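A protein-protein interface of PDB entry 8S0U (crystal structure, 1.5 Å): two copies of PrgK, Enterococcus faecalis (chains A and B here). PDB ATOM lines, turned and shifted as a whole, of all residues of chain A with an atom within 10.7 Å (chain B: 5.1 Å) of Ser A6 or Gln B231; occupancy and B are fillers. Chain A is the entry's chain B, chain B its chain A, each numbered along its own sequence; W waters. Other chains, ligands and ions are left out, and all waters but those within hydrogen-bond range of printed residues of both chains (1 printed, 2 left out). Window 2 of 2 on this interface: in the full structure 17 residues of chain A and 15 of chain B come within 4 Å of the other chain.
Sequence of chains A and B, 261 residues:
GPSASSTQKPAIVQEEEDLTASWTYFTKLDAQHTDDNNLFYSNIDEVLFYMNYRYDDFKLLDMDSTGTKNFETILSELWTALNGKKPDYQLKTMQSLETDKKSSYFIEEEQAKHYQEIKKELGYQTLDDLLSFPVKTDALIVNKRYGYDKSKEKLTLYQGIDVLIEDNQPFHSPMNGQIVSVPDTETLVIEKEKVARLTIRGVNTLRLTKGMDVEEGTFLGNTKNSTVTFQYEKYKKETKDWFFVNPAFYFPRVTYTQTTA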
ATOM      1  N   ALA A   4       3.958 -18.968  12.327  1.00  0.00           N
ATOM      2  CA  ALA A   4       3.843 -17.627  11.698  1.00  0.00           C
ATOM      3  C   ALA A   4       2.446 -17.421  11.150  1.00  0.00           C
ATOM      4  O   ALA A   4       1.803 -18.363  10.671  1.00  0.00           O
ATOM      5  CB  ALA A   4       4.860 -17.461  10.527  1.00  0.00           C
ATOM      6  N   SER A   5       1.986 -16.171  11.198  1.00  0.00           N
ATOM      7  CA  SER A   5       0.921 -15.744  10.298  1.00  0.00           C
ATOM      8  C   SER A   5       1.359 -15.823   8.839  1.00  0.00           C
ATOM      9  O   SER A   5       0.508 -15.928   7.947  1.00  0.00           O
ATOM     10  CB  SER A   5       0.481 -14.329  10.662  1.00  0.00           C
ATOM     11  OG  SER A   5       0.551 -14.128  12.064  1.00  0.00           O
ATOM     12  N   SER A   6       2.673 -15.785   8.560  1.00  0.00           N
ATOM     13  CA  SER A   6       3.167 -15.969   7.202  1.00  0.00           C
ATOM     14  C   SER A   6       3.284 -17.438   6.802  1.00  0.00           C
ATOM     15  O   SER A   6       3.514 -17.733   5.625  1.00  0.00           O
ATOM     16  CB  SER A   6       4.528 -15.277   7.010  1.00  0.00           C
ATOM     17  OG  SER A   6       5.018 -15.376   5.668  1.00  0.00           O
ATOM     18  N   THR A   7       3.105 -18.361   7.731  1.00  0.00           N
ATOM     19  CA  THR A   7       3.161 -19.786   7.450  1.00  0.00           C
ATOM     20  C   THR A   7       1.769 -20.324   7.134  1.00  0.00           C
ATOM     21  O   THR A   7       0.821 -20.083   7.885  1.00  0.00           O
ATOM     22  CB  THR A   7       3.708 -20.513   8.666  1.00  0.00           C
ATOM     23  OG1 THR A   7       5.065 -20.075   8.958  1.00  0.00           O
ATOM     24  CG2 THR A   7       3.705 -21.995   8.436  1.00  0.00           C
ATOM     25  N   GLN A   8       1.671 -21.092   6.057  1.00  0.00           N
ATOM     26  CA  GLN A   8       0.412 -21.672   5.595  1.00  0.00           C
ATOM     27  C   GLN A   8       0.599 -23.157   5.367  1.00  0.00           C
ATOM     28  O   GLN A   8       1.439 -23.566   4.574  1.00  0.00           O
ATOM     29  CB  GLN A   8      -0.046 -20.975   4.333  1.00  0.00           C
ATOM     30  CG  GLN A   8      -1.272 -21.569   3.651  1.00  0.00           C
ATOM     31  CD  GLN A   8      -2.487 -21.485   4.557  1.00  0.00           C
ATOM     32  OE1 GLN A   8      -2.937 -20.383   4.939  1.00  0.00           O
ATOM     33  NE2 GLN A   8      -2.993 -22.641   4.948  1.00  0.00           N
ATOM     34  N   LYS A   9      -0.171 -23.980   6.057  1.00  0.00           N
ATOM     35  CA  LYS A   9      -0.110 -25.415   5.795  1.00  0.00           C
ATOM     36  C   LYS A   9      -0.836 -25.731   4.492  1.00  0.00           C
ATOM     37  O   LYS A   9      -1.750 -25.017   4.060  1.00  0.00           O
ATOM     38  CB  LYS A   9      -0.705 -26.228   6.937  1.00  0.00           C
ATOM     39  CG  LYS A   9      -2.186 -26.192   7.084  1.00  0.00           C
ATOM     40  CD  LYS A   9      -2.610 -26.882   8.390  1.00  0.00           C
ATOM     41  CE  LYS A   9      -4.088 -27.267   8.363  1.00  0.00           C
ATOM     42  NZ  LYS A   9      -4.577 -27.642   9.743  1.00  0.00           N
ATOM     43  N   PRO A  10      -0.468 -26.815   3.819  1.00  0.00           N
ATOM     44  CA  PRO A  10      -1.181 -27.174   2.585  1.00  0.00           C
ATOM     45  C   PRO A  10      -2.617 -27.599   2.871  1.00  0.00           C
ATOM     46  O   PRO A  10      -3.003 -27.876   4.019  1.00  0.00           O
ATOM     47  CB  PRO A  10      -0.385 -28.349   2.030  1.00  0.00           C
ATOM     48  CG  PRO A  10       0.999 -28.205   2.671  1.00  0.00           C
ATOM     49  CD  PRO A  10       0.688 -27.686   4.053  1.00  0.00           C
ATOM     50  N   HIS A 114     -11.392 -19.548   5.076  1.00  0.00           N
ATOM     51  CA  HIS A 114      -9.977 -19.575   4.767  1.00  0.00           C
ATOM     52  C   HIS A 114      -9.535 -20.958   4.281  1.00  0.00           C
ATOM     53  O   HIS A 114      -8.799 -21.046   3.301  1.00  0.00           O
ATOM     54  CB  HIS A 114      -9.131 -19.153   5.968  1.00  0.00           C
ATOM     55  CG  HIS A 114      -7.680 -18.989   5.640  1.00  0.00           C
ATOM     56  ND1 HIS A 114      -7.078 -17.753   5.525  1.00  0.00           N
ATOM     57  CD2 HIS A 114      -6.709 -19.903   5.428  1.00  0.00           C
ATOM     58  CE1 HIS A 114      -5.801 -17.917   5.226  1.00  0.00           C
ATOM     59  NE2 HIS A 114      -5.551 -19.214   5.165  1.00  0.00           N
ATOM     60  N   ILE A 118      -7.915 -21.987   0.634  1.00  0.00           N
ATOM     61  CA  ILE A 118      -6.679 -22.746   0.445  1.00  0.00           C
ATOM     62  C   ILE A 118      -6.936 -24.008  -0.364  1.00  0.00           C
ATOM     63  O   ILE A 118      -6.115 -24.398  -1.206  1.00  0.00           O
ATOM     64  CB  ILE A 118      -6.030 -23.034   1.795  1.00  0.00           C
ATOM     65  CG1 ILE A 118      -5.638 -21.719   2.496  1.00  0.00           C
ATOM     66  CG2 ILE A 118      -4.833 -23.952   1.701  1.00  0.00           C
ATOM     67  CD1 ILE A 118      -4.679 -20.834   1.662  1.00  0.00           C
ATOM     68  N   LEU A 122      -4.735 -24.557  -3.641  1.00  0.00           N
ATOM     69  CA  LEU A 122      -3.748 -25.636  -3.621  1.00  0.00           C
ATOM     70  C   LEU A 122      -4.295 -26.998  -4.004  1.00  0.00           C
ATOM     71  O   LEU A 122      -3.565 -27.789  -4.611  1.00  0.00           O
ATOM     72  CB  LEU A 122      -3.084 -25.758  -2.254  1.00  0.00           C
ATOM     73  CG  LEU A 122      -2.449 -24.452  -1.704  1.00  0.00           C
ATOM     74  CD1 LEU A 122      -1.605 -24.767  -0.459  1.00  0.00           C
ATOM     75  CD2 LEU A 122      -1.631 -23.652  -2.702  1.00  0.00           C
ATOM     76  N   LEU B 157       4.115 -23.755   3.334  1.00  0.00           N
ATOM     77  CA  LEU B 157       4.262 -22.629   2.422  1.00  0.00           C
ATOM     78  C   LEU B 157       4.485 -21.361   3.225  1.00  0.00           C
ATOM     79  O   LEU B 157       3.714 -21.026   4.115  1.00  0.00           O
ATOM     80  CB  LEU B 157       2.986 -22.488   1.592  1.00  0.00           C
ATOM     81  CG  LEU B 157       2.867 -21.297   0.645  1.00  0.00           C
ATOM     82  CD1 LEU B 157       3.874 -21.278  -0.436  1.00  0.00           C
ATOM     83  CD2 LEU B 157       1.504 -21.315   0.010  1.00  0.00           C
ATOM     84  N   TYR B 158       5.551 -20.654   2.931  1.00  0.00           N
ATOM     85  CA  TYR B 158       5.894 -19.438   3.657  1.00  0.00           C
ATOM     86  C   TYR B 158       5.614 -18.265   2.740  1.00  0.00           C
ATOM     87  O   TYR B 158       6.311 -18.077   1.734  1.00  0.00           O
ATOM     88  CB  TYR B 158       7.331 -19.444   4.154  1.00  0.00           C
ATOM     89  CG  TYR B 158       7.602 -18.460   5.244  1.00  0.00           C
ATOM     90  CD1 TYR B 158       7.019 -18.599   6.489  1.00  0.00           C
ATOM     91  CD2 TYR B 158       8.445 -17.360   5.079  1.00  0.00           C
ATOM     92  CE1 TYR B 158       7.278 -17.757   7.512  1.00  0.00           C
ATOM     93  CE2 TYR B 158       8.708 -16.499   6.124  1.00  0.00           C
ATOM     94  CZ  TYR B 158       8.110 -16.690   7.353  1.00  0.00           C
ATOM     95  OH  TYR B 158       8.311 -15.853   8.411  1.00  0.00           O
ATOM     96  N   GLN B 159       4.628 -17.464   3.111  1.00  0.00           N
ATOM     97  CA  GLN B 159       4.151 -16.393   2.244  1.00  0.00           C
ATOM     98  C   GLN B 159       4.787 -15.052   2.546  1.00  0.00           C
ATOM     99  O   GLN B 159       4.136 -14.010   2.532  1.00  0.00           O
ATOM    100  CB  GLN B 159       2.621 -16.308   2.281  1.00  0.00           C
ATOM    101  CG  GLN B 159       2.011 -17.546   1.664  1.00  0.00           C
ATOM    102  CD  GLN B 159       0.478 -17.595   1.742  1.00  0.00           C
ATOM    103  OE1 GLN B 159      -0.181 -17.836   0.734  1.00  0.00           O
ATOM    104  NE2 GLN B 159      -0.057 -17.364   2.919  1.00  0.00           N
ATOM    105  N   GLY B 160       6.117 -15.054   2.697  1.00  0.00           N
ATOM    106  CA  GLY B 160       6.895 -13.858   2.930  1.00  0.00           C
ATOM    107  C   GLY B 160       8.357 -14.235   2.956  1.00  0.00           C
ATOM    108  O   GLY B 160       8.743 -15.307   2.473  1.00  0.00           O
ATOM    109  N   ARG B 197       0.214  -3.893  -0.625  1.00  0.00           N
ATOM    110  CA  ARG B 197       0.063  -3.976   0.826  1.00  0.00           C
ATOM    111  C   ARG B 197       1.293  -4.681   1.387  1.00  0.00           C
ATOM    112  O   ARG B 197       1.550  -5.832   1.017  1.00  0.00           O
ATOM    113  CB  ARG B 197      -1.218  -4.751   1.178  1.00  0.00           C
ATOM    114  CG  ARG B 197      -1.616  -4.678   2.621  1.00  0.00           C
ATOM    115  CD  ARG B 197      -3.102  -5.062   2.774  1.00  0.00           C
ATOM    116  NE  ARG B 197      -3.362  -6.435   2.404  1.00  0.00           N
ATOM    117  CZ  ARG B 197      -4.573  -6.911   2.131  1.00  0.00           C
ATOM    118  NH1 ARG B 197      -5.628  -6.117   2.062  1.00  0.00           N
ATOM    119  NH2 ARG B 197      -4.728  -8.213   1.904  1.00  0.00           N
ATOM    120  N   LEU B 198       2.003  -4.014   2.274  1.00  0.00           N
ATOM    121  CA  LEU B 198       3.211  -4.552   2.911  1.00  0.00           C
ATOM    122  C   LEU B 198       2.981  -4.766   4.400  1.00  0.00           C
ATOM    123  O   LEU B 198       2.576  -3.856   5.117  1.00  0.00           O
ATOM    124  CB  LEU B 198       4.370  -3.581   2.712  1.00  0.00           C
ATOM    125  CG  LEU B 198       5.748  -3.987   3.264  1.00  0.00           C
ATOM    126  CD1 LEU B 198       6.258  -5.132   2.520  1.00  0.00           C
ATOM    127  CD2 LEU B 198       6.700  -2.846   3.297  1.00  0.00           C
ATOM    128  N   THR B 199       3.204  -6.012   4.850  1.00  0.00           N
ATOM    129  CA  THR B 199       3.135  -6.369   6.261  1.00  0.00           C
ATOM    130  C   THR B 199       4.555  -6.489   6.779  1.00  0.00           C
ATOM    131  O   THR B 199       5.376  -7.165   6.156  1.00  0.00           O
ATOM    132  CB  THR B 199       2.386  -7.692   6.410  1.00  0.00           C
ATOM    133  OG1 THR B 199       1.074  -7.581   5.811  1.00  0.00           O
ATOM    134  CG2 THR B 199       2.214  -8.064   7.891  1.00  0.00           C
ATOM    135  N   ARG B 201       6.773  -7.457  10.242  1.00  0.00           N
ATOM    136  CA  ARG B 201       6.747  -8.051  11.577  1.00  0.00           C
ATOM    137  C   ARG B 201       8.141  -7.956  12.173  1.00  0.00           C
ATOM    138  O   ARG B 201       9.116  -8.421  11.565  1.00  0.00           O
ATOM    139  CB  ARG B 201       6.319  -9.513  11.537  1.00  0.00           C
ATOM    140  CG  ARG B 201       4.895  -9.740  10.932  1.00  0.00           C
ATOM    141  CD  ARG B 201       4.704 -11.208  10.496  1.00  0.00           C
ATOM    142  NE  ARG B 201       3.531 -11.413   9.640  1.00  0.00           N
ATOM    143  CZ  ARG B 201       2.283 -11.270  10.070  1.00  0.00           C
ATOM    144  NH1 ARG B 201       2.021 -10.924  11.320  1.00  0.00           N
ATOM    145  NH2 ARG B 201       1.274 -11.465   9.225  1.00  0.00           N
ATOM    146  N   THR B 229      10.159  -9.952   9.368  1.00  0.00           N
ATOM    147  CA  THR B 229       9.424 -10.657   8.319  1.00  0.00           C
ATOM    148  C   THR B 229       8.655  -9.648   7.474  1.00  0.00           C
ATOM    149  O   THR B 229       8.032  -8.734   8.011  1.00  0.00           O
ATOM    150  CB  THR B 229       8.445 -11.687   8.903  1.00  0.00           C
ATOM    151  OG1 THR B 229       9.202 -12.672   9.634  1.00  0.00           O
ATOM    152  CG2 THR B 229       7.608 -12.365   7.822  1.00  0.00           C
ATOM    153  N   PHE B 230       8.758  -9.793   6.149  1.00  0.00           N
ATOM    154  CA  PHE B 230       7.975  -9.014   5.190  1.00  0.00           C
ATOM    155  C   PHE B 230       7.025  -9.948   4.458  1.00  0.00           C
ATOM    156  O   PHE B 230       7.410 -11.039   4.020  1.00  0.00           O
ATOM    157  CB  PHE B 230       8.845  -8.385   4.098  1.00  0.00           C
ATOM    158  CG  PHE B 230       9.751  -7.312   4.583  1.00  0.00           C
ATOM    159  CD1 PHE B 230       9.246  -6.102   4.986  1.00  0.00           C
ATOM    160  CD2 PHE B 230      11.120  -7.496   4.560  1.00  0.00           C
ATOM    161  CE1 PHE B 230      10.094  -5.079   5.413  1.00  0.00           C
ATOM    162  CE2 PHE B 230      11.978  -6.470   4.993  1.00  0.00           C
ATOM    163  CZ  PHE B 230      11.462  -5.272   5.404  1.00  0.00           C
ATOM    164  N   GLN B 231       5.801  -9.479   4.286  1.00  0.00           N
ATOM    165  CA  GLN B 231       4.862 -10.043   3.337  1.00  0.00           C
ATOM    166  C   GLN B 231       4.403  -8.906   2.459  1.00  0.00           C
ATOM    167  O   GLN B 231       4.253  -7.764   2.920  1.00  0.00           O
ATOM    168  CB  GLN B 231       3.630 -10.614   4.087  1.00  0.00           C
ATOM    169  CG  GLN B 231       3.945 -11.780   4.958  1.00  0.00           C
ATOM    170  CD  GLN B 231       2.704 -12.473   5.467  1.00  0.00           C
ATOM    171  OE1 GLN B 231       2.128 -12.107   6.504  1.00  0.00           O
ATOM    172  NE2 GLN B 231       2.257 -13.430   4.716  1.00  0.00           N
ATOM    173  N   TYR B 232       4.183  -9.210   1.195  1.00  0.00           N
ATOM    174  CA  TYR B 232       3.838  -8.201   0.194  1.00  0.00           C
ATOM    175  C   TYR B 232       2.754  -8.771  -0.700  1.00  0.00           C
ATOM    176  O   TYR B 232       2.845  -9.914  -1.153  1.00  0.00           O
ATOM    177  CB  TYR B 232       5.098  -7.826  -0.595  1.00  0.00           C
ATOM    178  CG  TYR B 232       5.047  -6.511  -1.356  1.00  0.00           C
ATOM    179  CD1 TYR B 232       4.399  -5.407  -0.831  1.00  0.00           C
ATOM    180  CD2 TYR B 232       5.724  -6.368  -2.571  1.00  0.00           C
ATOM    181  CE1 TYR B 232       4.414  -4.174  -1.512  1.00  0.00           C
ATOM    182  CE2 TYR B 232       5.757  -5.159  -3.246  1.00  0.00           C
ATOM    183  CZ  TYR B 232       5.093  -4.059  -2.709  1.00  0.00           C
ATOM    184  OH  TYR B 232       5.086  -2.833  -3.341  1.00  0.00           O
ATOM    185  N   GLU B 233       1.726  -7.964  -0.935  1.00  0.00           N
ATOM    186  CA  GLU B 233       0.585  -8.355  -1.730  1.00  0.00           C
ATOM    187  C   GLU B 233       0.271  -7.271  -2.751  1.00  0.00           C
ATOM    188  O   GLU B 233       0.522  -6.085  -2.525  1.00  0.00           O
ATOM    189  CB  GLU B 233      -0.645  -8.502  -0.862  1.00  0.00           C
ATOM    190  CG  GLU B 233      -0.514  -9.606   0.145  1.00  0.00           C
ATOM    191  CD  GLU B 233      -1.611  -9.501   1.198  1.00  0.00           C
ATOM    192  OE1 GLU B 233      -1.422  -8.757   2.200  1.00  0.00           O
ATOM    193  OE2 GLU B 233      -2.696 -10.103   0.968  1.00  0.00           O
ATOM    194  N   PHE B 244      -0.461 -12.740  -2.811  1.00  0.00           N
ATOM    195  CA  PHE B 244       0.917 -12.609  -2.309  1.00  0.00           C
ATOM    196  C   PHE B 244       1.918 -12.625  -3.466  1.00  0.00           C
ATOM    197  O   PHE B 244       1.743 -13.304  -4.493  1.00  0.00           O
ATOM    198  CB  PHE B 244       1.229 -13.734  -1.315  1.00  0.00           C
ATOM    199  CG  PHE B 244       0.558 -13.573  -0.019  1.00  0.00           C
ATOM    200  CD1 PHE B 244       0.971 -12.593   0.866  1.00  0.00           C
ATOM    201  CD2 PHE B 244      -0.506 -14.402   0.338  1.00  0.00           C
ATOM    202  CE1 PHE B 244       0.348 -12.408   2.074  1.00  0.00           C
ATOM    203  CE2 PHE B 244      -1.150 -14.217   1.554  1.00  0.00           C
ATOM    204  CZ  PHE B 244      -0.727 -13.241   2.427  1.00  0.00           C
ATOM    205  N   PRO B 247       8.407 -10.967  -1.779  1.00  0.00           N
ATOM    206  CA  PRO B 247       8.932  -9.632  -1.512  1.00  0.00           C
ATOM    207  C   PRO B 247      10.339  -9.442  -2.010  1.00  0.00           C
ATOM    208  O   PRO B 247      10.749  -8.312  -2.262  1.00  0.00           O
ATOM    209  CB  PRO B 247       8.847  -9.507   0.031  1.00  0.00           C
ATOM    210  CG  PRO B 247       7.799 -10.514   0.422  1.00  0.00           C
ATOM    211  CD  PRO B 247       7.995 -11.653  -0.524  1.00  0.00           C
HETATM  212  O   HOH W   1       0.061 -15.293   5.165  1.00  0.00           O
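Printed residues of chain A that touch a printed residue of chain B: Ala A4, Ser A5, Ser A6, Thr A7 and Gln A8. Hydrophobic or aromatic side chains of chain A that line the printed part of chain B: Ala A4. Hydrophobic or aromatic side chains of chain B that line the printed part of chain A: Leu B157 and Tyr B158. Among the printed residues, no Asp or Glu carboxylate lies within 4 Å of a Lys or Arg side-chain nitrogen of the other chain.
No position is printed for both chains.
OG of Ser A6 is in hydrogen-bond range of N of Gly B160 (3.2 Å). N of Gln B159 sits at hydrogen-bond distance from O of Ser A6 (2.8 Å). The backbone carbonyl oxygen (O) of Leu B157 lies within hydrogen-bond range of the backbone NH (N) of Gln A8 (2.8 Å).
Water W1 lies within hydrogen-bond range of O of Ser A5 (2.9 Å), NE2 of Gln B231 (2.9 Å) and NE2 of Gln B159 (3.1 Å).
Printed residues of chain B within 4 Å of Ser A6: Leu B157, Tyr B158, Gln B159, Gly B160 and Gln B231. Printed residues of chain A within 4 Å of Gln B231: Ser A6. No residue of chain A comes within 4 Å of Leu B198. Of the printed residues of chain A, Tyr B158 touches Ala A4 (3.9 Å), Ser A6 (3.5 Å) and Thr A7 (3.5 Å). Printed residues of chain B within 4 Å of Ala A4: Tyr B158 (3.9 Å). Of the printed residues of chain B, Ser A5 touches Arg B201. Of the printed residues of chain A, Gln B159 touches Ser A6 and Gln A8. Pro B247 touches none of the printed residues of chain A. Phe B244 touches none of the printed residues of chain A. The nearest printed residue of chain A that does not touch Gly B160 is Thr A7 (6.7 Å).
OE1 of Gln A8 lies within hydrogen-bond range of NE2 of His A114 (2.9 Å). The backbone carbonyl oxygen of Gln B231 sits at hydrogen-bond distance from the backbone NH of Thr B199, 2.8 Å away. The backbone carbonyl oxygen (O) of Gln B159 sits at hydrogen-bond distance from the side-chain amide nitrogen (NE2) of Gln B231, 2.9 Å away. The guanidinium group (NH2) of Arg B201 is in hydrogen-bond range of the side-chain amide oxygen (OE1) of Gln B231, 2.9 Å away. N of Arg B201 sits at hydrogen-bond distance from O of Thr B229, at 2.9 Å.
Among the printed residues, pairs that only touch across the chains: Ala A4 with Tyr B158 (3.9 Å), Ser A5 with Arg B201 (3.3 Å), Ser A6 with Leu B157 (3.6 Å), Ser A6 with Tyr B158 (3.5 Å), Ser A6 with Gln B231 (3.5 Å), Thr A7 with Leu B157 (3.6 Å), Thr A7 with Tyr B158 (3.5 Å) and Gln A8 with Gln B159 (3.9 Å).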
